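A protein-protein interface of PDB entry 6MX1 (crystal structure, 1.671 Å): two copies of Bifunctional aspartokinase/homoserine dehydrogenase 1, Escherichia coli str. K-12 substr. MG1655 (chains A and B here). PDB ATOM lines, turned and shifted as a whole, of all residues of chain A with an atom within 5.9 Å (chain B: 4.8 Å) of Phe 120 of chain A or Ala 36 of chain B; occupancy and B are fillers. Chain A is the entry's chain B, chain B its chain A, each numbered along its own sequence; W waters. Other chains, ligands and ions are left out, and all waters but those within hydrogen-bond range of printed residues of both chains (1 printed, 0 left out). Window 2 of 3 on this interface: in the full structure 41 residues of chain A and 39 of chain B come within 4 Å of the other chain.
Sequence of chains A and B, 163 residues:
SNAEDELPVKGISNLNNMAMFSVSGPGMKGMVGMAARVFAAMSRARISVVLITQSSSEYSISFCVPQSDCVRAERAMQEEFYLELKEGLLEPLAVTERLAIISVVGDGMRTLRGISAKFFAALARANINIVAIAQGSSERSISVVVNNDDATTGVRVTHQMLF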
ATOM      1  N   ILE A 115     -28.626 -36.361  23.356  1.00  0.00           N
ATOM      2  CA  ILE A 115     -27.211 -36.596  23.617  1.00  0.00           C
ATOM      3  C   ILE A 115     -26.370 -35.423  23.130  1.00  0.00           C
ATOM      4  O   ILE A 115     -25.577 -34.857  23.892  1.00  0.00           O
ATOM      5  CB  ILE A 115     -26.752 -37.917  22.979  1.00  0.00           C
ATOM      6  CG1 ILE A 115     -27.258 -39.112  23.774  1.00  0.00           C
ATOM      7  CG2 ILE A 115     -25.247 -37.974  22.949  1.00  0.00           C
ATOM      8  CD1 ILE A 115     -27.221 -38.903  25.270  1.00  0.00           C
ATOM      9  N   SER A 116     -26.501 -35.048  21.850  1.00  0.00           N
ATOM     10  CA  SER A 116     -25.625 -34.000  21.325  1.00  0.00           C
ATOM     11  C   SER A 116     -25.855 -32.683  22.053  1.00  0.00           C
ATOM     12  O   SER A 116     -24.893 -31.975  22.369  1.00  0.00           O
ATOM     13  CB  SER A 116     -25.792 -33.834  19.811  1.00  0.00           C
ATOM     14  OG  SER A 116     -24.964 -34.759  19.115  1.00  0.00           O
ATOM     15  N   ALA A 117     -27.111 -32.372  22.381  1.00  0.00           N
ATOM     16  CA  ALA A 117     -27.406 -31.167  23.148  1.00  0.00           C
ATOM     17  C   ALA A 117     -26.677 -31.172  24.492  1.00  0.00           C
ATOM     18  O   ALA A 117     -26.022 -30.191  24.845  1.00  0.00           O
ATOM     19  CB  ALA A 117     -28.908 -31.033  23.366  1.00  0.00           C
ATOM     20  N   LYS A 118     -26.792 -32.268  25.247  1.00  0.00           N
ATOM     21  CA  LYS A 118     -26.218 -32.306  26.592  1.00  0.00           C
ATOM     22  C   LYS A 118     -24.697 -32.377  26.554  1.00  0.00           C
ATOM     23  O   LYS A 118     -24.016 -31.801  27.420  1.00  0.00           O
ATOM     24  CB  LYS A 118     -26.797 -33.486  27.373  1.00  0.00           C
ATOM     25  CG  LYS A 118     -28.281 -33.389  27.732  1.00  0.00           C
ATOM     26  CD  LYS A 118     -28.698 -34.667  28.464  1.00  0.00           C
ATOM     27  CE  LYS A 118     -30.135 -34.676  28.944  1.00  0.00           C
ATOM     28  NZ  LYS A 118     -31.093 -35.046  27.877  1.00  0.00           N
ATOM     29  N   PHE A 119     -24.146 -33.112  25.579  1.00  0.00           N
ATOM     30  CA  PHE A 119     -22.694 -33.159  25.389  1.00  0.00           C
ATOM     31  C   PHE A 119     -22.131 -31.747  25.187  1.00  0.00           C
ATOM     32  O   PHE A 119     -21.218 -31.315  25.905  1.00  0.00           O
ATOM     33  CB  PHE A 119     -22.400 -34.101  24.204  1.00  0.00           C
ATOM     34  CG  PHE A 119     -20.919 -34.272  23.839  1.00  0.00           C
ATOM     35  CD1 PHE A 119     -19.925 -34.282  24.785  1.00  0.00           C
ATOM     36  CD2 PHE A 119     -20.530 -34.420  22.509  1.00  0.00           C
ATOM     37  CE1 PHE A 119     -18.576 -34.425  24.413  1.00  0.00           C
ATOM     38  CE2 PHE A 119     -19.149 -34.565  22.147  1.00  0.00           C
ATOM     39  CZ  PHE A 119     -18.194 -34.569  23.089  1.00  0.00           C
ATOM     40  N   PHE A 120     -22.695 -30.990  24.232  1.00  0.00           N
ATOM     41  CA  PHE A 120     -22.250 -29.615  24.006  1.00  0.00           C
ATOM     42  C   PHE A 120     -22.552 -28.735  25.219  1.00  0.00           C
ATOM     43  O   PHE A 120     -21.762 -27.851  25.555  1.00  0.00           O
ATOM     44  CB  PHE A 120     -22.905 -29.040  22.748  1.00  0.00           C
ATOM     45  CG  PHE A 120     -22.339 -29.605  21.471  1.00  0.00           C
ATOM     46  CD1 PHE A 120     -21.022 -29.385  21.157  1.00  0.00           C
ATOM     47  CD2 PHE A 120     -23.123 -30.374  20.622  1.00  0.00           C
ATOM     48  CE1 PHE A 120     -20.489 -29.909  19.984  1.00  0.00           C
ATOM     49  CE2 PHE A 120     -22.586 -30.906  19.447  1.00  0.00           C
ATOM     50  CZ  PHE A 120     -21.235 -30.675  19.171  1.00  0.00           C
ATOM     51  N   ALA A 121     -23.685 -28.950  25.883  1.00  0.00           N
ATOM     52  CA  ALA A 121     -23.946 -28.210  27.121  1.00  0.00           C
ATOM     53  C   ALA A 121     -22.864 -28.459  28.182  1.00  0.00           C
ATOM     54  O   ALA A 121     -22.434 -27.516  28.867  1.00  0.00           O
ATOM     55  CB  ALA A 121     -25.325 -28.578  27.667  1.00  0.00           C
ATOM     56  N   ALA A 122     -22.426 -29.718  28.344  1.00  0.00           N
ATOM     57  CA  ALA A 122     -21.422 -30.017  29.378  1.00  0.00           C
ATOM     58  C   ALA A 122     -20.110 -29.325  29.074  1.00  0.00           C
ATOM     59  O   ALA A 122     -19.465 -28.779  29.985  1.00  0.00           O
ATOM     60  CB  ALA A 122     -21.197 -31.520  29.498  1.00  0.00           C
ATOM     61  N   LEU A 123     -19.702 -29.326  27.794  1.00  0.00           N
ATOM     62  CA  LEU A 123     -18.445 -28.694  27.446  1.00  0.00           C
ATOM     63  C   LEU A 123     -18.536 -27.189  27.607  1.00  0.00           C
ATOM     64  O   LEU A 123     -17.573 -26.556  28.058  1.00  0.00           O
ATOM     65  CB  LEU A 123     -18.013 -29.066  26.032  1.00  0.00           C
ATOM     66  CG  LEU A 123     -17.786 -30.544  25.719  1.00  0.00           C
ATOM     67  CD1 LEU A 123     -17.500 -30.660  24.209  1.00  0.00           C
ATOM     68  CD2 LEU A 123     -16.637 -31.171  26.558  1.00  0.00           C
ATOM     69  N   ALA A 124     -19.682 -26.594  27.257  1.00  0.00           N
ATOM     70  CA  ALA A 124     -19.838 -25.151  27.416  1.00  0.00           C
ATOM     71  C   ALA A 124     -19.803 -24.747  28.893  1.00  0.00           C
ATOM     72  O   ALA A 124     -19.155 -23.763  29.257  1.00  0.00           O
ATOM     73  CB  ALA A 124     -21.137 -24.692  26.769  1.00  0.00           C
ATOM     74  N   ARG A 125     -20.504 -25.500  29.739  1.00  0.00           N
ATOM     75  CA  ARG A 125     -20.480 -25.292  31.193  1.00  0.00           C
ATOM     76  C   ARG A 125     -19.062 -25.322  31.749  1.00  0.00           C
ATOM     77  O   ARG A 125     -18.748 -24.590  32.703  1.00  0.00           O
ATOM     78  CB  ARG A 125     -21.358 -26.364  31.845  1.00  0.00           C
ATOM     79  CG  ARG A 125     -21.042 -26.706  33.296  1.00  0.00           C
ATOM     80  CD  ARG A 125     -22.149 -27.575  33.910  1.00  0.00           C
ATOM     81  NE  ARG A 125     -23.442 -26.886  33.949  1.00  0.00           N
ATOM     82  CZ  ARG A 125     -23.852 -26.100  34.950  1.00  0.00           C
ATOM     83  NH1 ARG A 125     -23.063 -25.883  35.997  1.00  0.00           N
ATOM     84  NH2 ARG A 125     -25.049 -25.513  34.901  1.00  0.00           N
ATOM     85  N   ILE A 130     -14.401 -25.289  21.585  1.00  0.00           N
ATOM     86  CA  ILE A 130     -14.528 -26.316  20.547  1.00  0.00           C
ATOM     87  C   ILE A 130     -13.726 -25.870  19.333  1.00  0.00           C
ATOM     88  O   ILE A 130     -13.901 -24.749  18.846  1.00  0.00           O
ATOM     89  CB  ILE A 130     -16.003 -26.553  20.214  1.00  0.00           C
ATOM     90  CG1 ILE A 130     -16.598 -27.284  21.398  1.00  0.00           C
ATOM     91  CG2 ILE A 130     -16.140 -27.355  18.941  1.00  0.00           C
ATOM     92  CD1 ILE A 130     -18.082 -27.503  21.362  1.00  0.00           C
ATOM     93  N   ILE A 133     -16.027 -29.924  14.840  1.00  0.00           N
ATOM     94  CA  ILE A 133     -17.052 -30.899  15.178  1.00  0.00           C
ATOM     95  C   ILE A 133     -17.220 -31.806  13.979  1.00  0.00           C
ATOM     96  O   ILE A 133     -17.256 -31.311  12.835  1.00  0.00           O
ATOM     97  CB  ILE A 133     -18.382 -30.216  15.485  1.00  0.00           C
ATOM     98  CG1 ILE A 133     -18.264 -29.308  16.688  1.00  0.00           C
ATOM     99  CG2 ILE A 133     -19.478 -31.251  15.757  1.00  0.00           C
ATOM    100  CD1 ILE A 133     -19.499 -28.413  16.808  1.00  0.00           C
ATOM    101  N   ILE A 142     -20.571 -38.716  17.845  1.00  0.00           N
ATOM    102  CA  ILE A 142     -20.210 -37.342  17.585  1.00  0.00           C
ATOM    103  C   ILE A 142     -18.816 -37.111  18.142  1.00  0.00           C
ATOM    104  O   ILE A 142     -18.519 -37.542  19.269  1.00  0.00           O
ATOM    105  CB  ILE A 142     -21.208 -36.358  18.209  1.00  0.00           C
ATOM    106  CG1 ILE A 142     -20.695 -34.932  18.005  1.00  0.00           C
ATOM    107  CG2 ILE A 142     -21.458 -36.679  19.630  1.00  0.00           C
ATOM    108  CD1 ILE A 142     -21.758 -33.907  17.982  1.00  0.00           C
ATOM    109  N   VAL A 144     -15.646 -34.283  18.867  1.00  0.00           N
ATOM    110  CA  VAL A 144     -15.392 -32.857  18.987  1.00  0.00           C
ATOM    111  C   VAL A 144     -13.905 -32.688  19.243  1.00  0.00           C
ATOM    112  O   VAL A 144     -13.341 -33.456  20.021  1.00  0.00           O
ATOM    113  CB  VAL A 144     -16.247 -32.246  20.110  1.00  0.00           C
ATOM    114  CG1 VAL A 144     -15.872 -30.778  20.377  1.00  0.00           C
ATOM    115  CG2 VAL A 144     -17.716 -32.349  19.727  1.00  0.00           C
ATOM    116  N   GLY B  33     -20.720 -21.439  23.648  1.00  0.00           N
ATOM    117  CA  GLY B  33     -21.814 -22.377  23.681  1.00  0.00           C
ATOM    118  C   GLY B  33     -22.729 -22.285  22.482  1.00  0.00           C
ATOM    119  O   GLY B  33     -23.918 -22.605  22.595  1.00  0.00           O
ATOM    120  N   MET B  34     -22.194 -21.843  21.328  1.00  0.00           N
ATOM    121  CA  MET B  34     -22.998 -21.674  20.128  1.00  0.00           C
ATOM    122  C   MET B  34     -23.581 -23.005  19.659  1.00  0.00           C
ATOM    123  O   MET B  34     -24.798 -23.124  19.456  1.00  0.00           O
ATOM    124  CB  MET B  34     -22.149 -21.018  19.035  1.00  0.00           C
ATOM    125  CG  MET B  34     -22.930 -20.339  17.893  1.00  0.00           C
ATOM    126  SD  MET B  34     -23.888 -18.815  18.220  1.00  0.00           S
ATOM    127  CE  MET B  34     -23.402 -18.260  19.861  1.00  0.00           C
ATOM    128  N   ALA B  35     -22.743 -24.034  19.533  1.00  0.00           N
ATOM    129  CA  ALA B  35     -23.267 -25.360  19.213  1.00  0.00           C
ATOM    130  C   ALA B  35     -24.267 -25.838  20.277  1.00  0.00           C
ATOM    131  O   ALA B  35     -25.335 -26.388  19.938  1.00  0.00           O
ATOM    132  CB  ALA B  35     -22.110 -26.353  19.061  1.00  0.00           C
ATOM    133  N   ALA B  36     -23.948 -25.653  21.575  1.00  0.00           N
ATOM    134  CA  ALA B  36     -24.911 -26.075  22.593  1.00  0.00           C
ATOM    135  C   ALA B  36     -26.276 -25.411  22.389  1.00  0.00           C
ATOM    136  O   ALA B  36     -27.322 -26.063  22.564  1.00  0.00           O
ATOM    137  CB  ALA B  36     -24.327 -25.779  23.986  1.00  0.00           C
ATOM    138  N   ARG B  37     -26.296 -24.127  22.009  1.00  0.00           N
ATOM    139  CA  ARG B  37     -27.578 -23.438  21.790  1.00  0.00           C
ATOM    140  C   ARG B  37     -28.298 -23.961  20.568  1.00  0.00           C
ATOM    141  O   ARG B  37     -29.532 -24.111  20.602  1.00  0.00           O
ATOM    142  CB  ARG B  37     -27.386 -21.940  21.627  1.00  0.00           C
ATOM    143  CG  ARG B  37     -27.109 -21.268  22.993  1.00  0.00           C
ATOM    144  CD  ARG B  37     -26.738 -19.825  22.754  1.00  0.00           C
ATOM    145  NE  ARG B  37     -27.861 -19.016  22.296  1.00  0.00           N
ATOM    146  CZ  ARG B  37     -27.718 -17.778  21.858  1.00  0.00           C
ATOM    147  NH1 ARG B  37     -26.504 -17.240  21.841  1.00  0.00           N
ATOM    148  NH2 ARG B  37     -28.763 -17.063  21.458  1.00  0.00           N
ATOM    149  N   VAL B  38     -27.552 -24.190  19.486  1.00  0.00           N
ATOM    150  CA  VAL B  38     -28.141 -24.711  18.232  1.00  0.00           C
ATOM    151  C   VAL B  38     -28.829 -26.036  18.536  1.00  0.00           C
ATOM    152  O   VAL B  38     -30.011 -26.261  18.214  1.00  0.00           O
ATOM    153  CB  VAL B  38     -27.060 -24.875  17.144  1.00  0.00           C
ATOM    154  CG1 VAL B  38     -27.609 -25.619  15.928  1.00  0.00           C
ATOM    155  CG2 VAL B  38     -26.522 -23.550  16.682  1.00  0.00           C
ATOM    156  N   PHE B  39     -28.122 -26.909  19.243  1.00  0.00           N
ATOM    157  CA  PHE B  39     -28.679 -28.231  19.392  1.00  0.00           C
ATOM    158  C   PHE B  39     -29.676 -28.333  20.539  1.00  0.00           C
ATOM    159  O   PHE B  39     -30.572 -29.189  20.472  1.00  0.00           O
ATOM    160  CB  PHE B  39     -27.507 -29.208  19.425  1.00  0.00           C
ATOM    161  CG  PHE B  39     -26.763 -29.166  18.125  1.00  0.00           C
ATOM    162  CD1 PHE B  39     -27.486 -29.295  16.934  1.00  0.00           C
ATOM    163  CD2 PHE B  39     -25.425 -28.853  18.055  1.00  0.00           C
ATOM    164  CE1 PHE B  39     -26.864 -29.200  15.690  1.00  0.00           C
ATOM    165  CE2 PHE B  39     -24.789 -28.751  16.817  1.00  0.00           C
ATOM    166  CZ  PHE B  39     -25.509 -28.919  15.634  1.00  0.00           C
ATOM    167  N   ALA B  40     -29.646 -27.407  21.516  1.00  0.00           N
ATOM    168  CA  ALA B  40     -30.770 -27.328  22.438  1.00  0.00           C
ATOM    169  C   ALA B  40     -32.028 -26.862  21.708  1.00  0.00           C
ATOM    170  O   ALA B  40     -33.131 -27.314  22.029  1.00  0.00           O
ATOM    171  CB  ALA B  40     -30.454 -26.407  23.624  1.00  0.00           C
ATOM    172  N   ILE B  52     -23.610 -33.192  11.617  1.00  0.00           N
ATOM    173  CA  ILE B  52     -23.162 -31.897  12.126  1.00  0.00           C
ATOM    174  C   ILE B  52     -21.708 -31.756  11.758  1.00  0.00           C
ATOM    175  O   ILE B  52     -20.938 -32.707  11.890  1.00  0.00           O
ATOM    176  CB  ILE B  52     -23.244 -31.727  13.663  1.00  0.00           C
ATOM    177  CG1 ILE B  52     -24.601 -32.109  14.171  1.00  0.00           C
ATOM    178  CG2 ILE B  52     -22.901 -30.207  14.025  1.00  0.00           C
ATOM    179  CD1 ILE B  52     -24.635 -32.149  15.672  1.00  0.00           C
HETATM  180  O   HOH W   1     -27.254 -27.957  24.672  1.00  0.00           O
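Hydrophobic or aromatic side chains of chain B that line the printed part of chain A: Ala 35, Ala 36, Phe 39 and Ile 52.
Of the 15 printed residues of chain A, 5 touch a printed residue of chain B.
Printed residues of chain A that touch a printed residue of chain B: Ala 117, Phe 120, Ala 121, Ala 124 and Ile 133.
Hydrophobic or aromatic side chains of chain A within 4 Å of the printed part of chain B: Ala 117, Phe 120, Ala 124 and Ile 133.
Among the printed residues, no Asp or Glu carboxylate lies within 4 Å of a Lys or Arg side-chain nitrogen of the other chain.
Water W1 lies within hydrogen-bond range of O of Ala 117 of chain A and O of Ala 36 of chain B.
Among the printed residues, merely in contact across the chains: Phe 120 of chain A with Ala 36 of chain B, Ala 121 of chain A with Ala 36 of chain B, Phe 120 of chain A with Phe 39 of chain B, Ala 117 of chain A with Phe 39 of chain B, Phe 120 of chain A with Ala 35 of chain B, Ala 124 of chain A with Gly 33 of chain B and Ile 133 of chain A with Ile 52 of chain B.
No position is printed for both chains.
Ser 116 of chain A touches none of the printed residues of chain B.
Printed residues of chain B within 4 Å of Ala 117 of chain A: Phe 39 (3.8 Å).
Printed residues of chain B within 4 Å of Phe 120 of chain A: Ala 35 (3.8 Å), Ala 36 (3.6 Å) and Phe 39 (3.8 Å).
Val 144 of chain A touches none of the printed residues of chain B.
Printed residues of chain A within 4 Å of Gly 33 of chain B: Ala 124.
Printed residues of chain A within 4 Å of Ala 35 of chain B: Phe 120 (3.8 Å).
Of the printed residues of chain A, Ala 36 of chain B touches Phe 120 (3.6 Å) and Ala 121 (3.8 Å).
The nearest residue of chain A that does not touch Ala 36 of chain B is Ala 124 of chain A (4.4 Å).
The nearest printed residue of chain A that does not touch Ile 52 of chain B is Ile 142 of chain A (4.1 Å).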
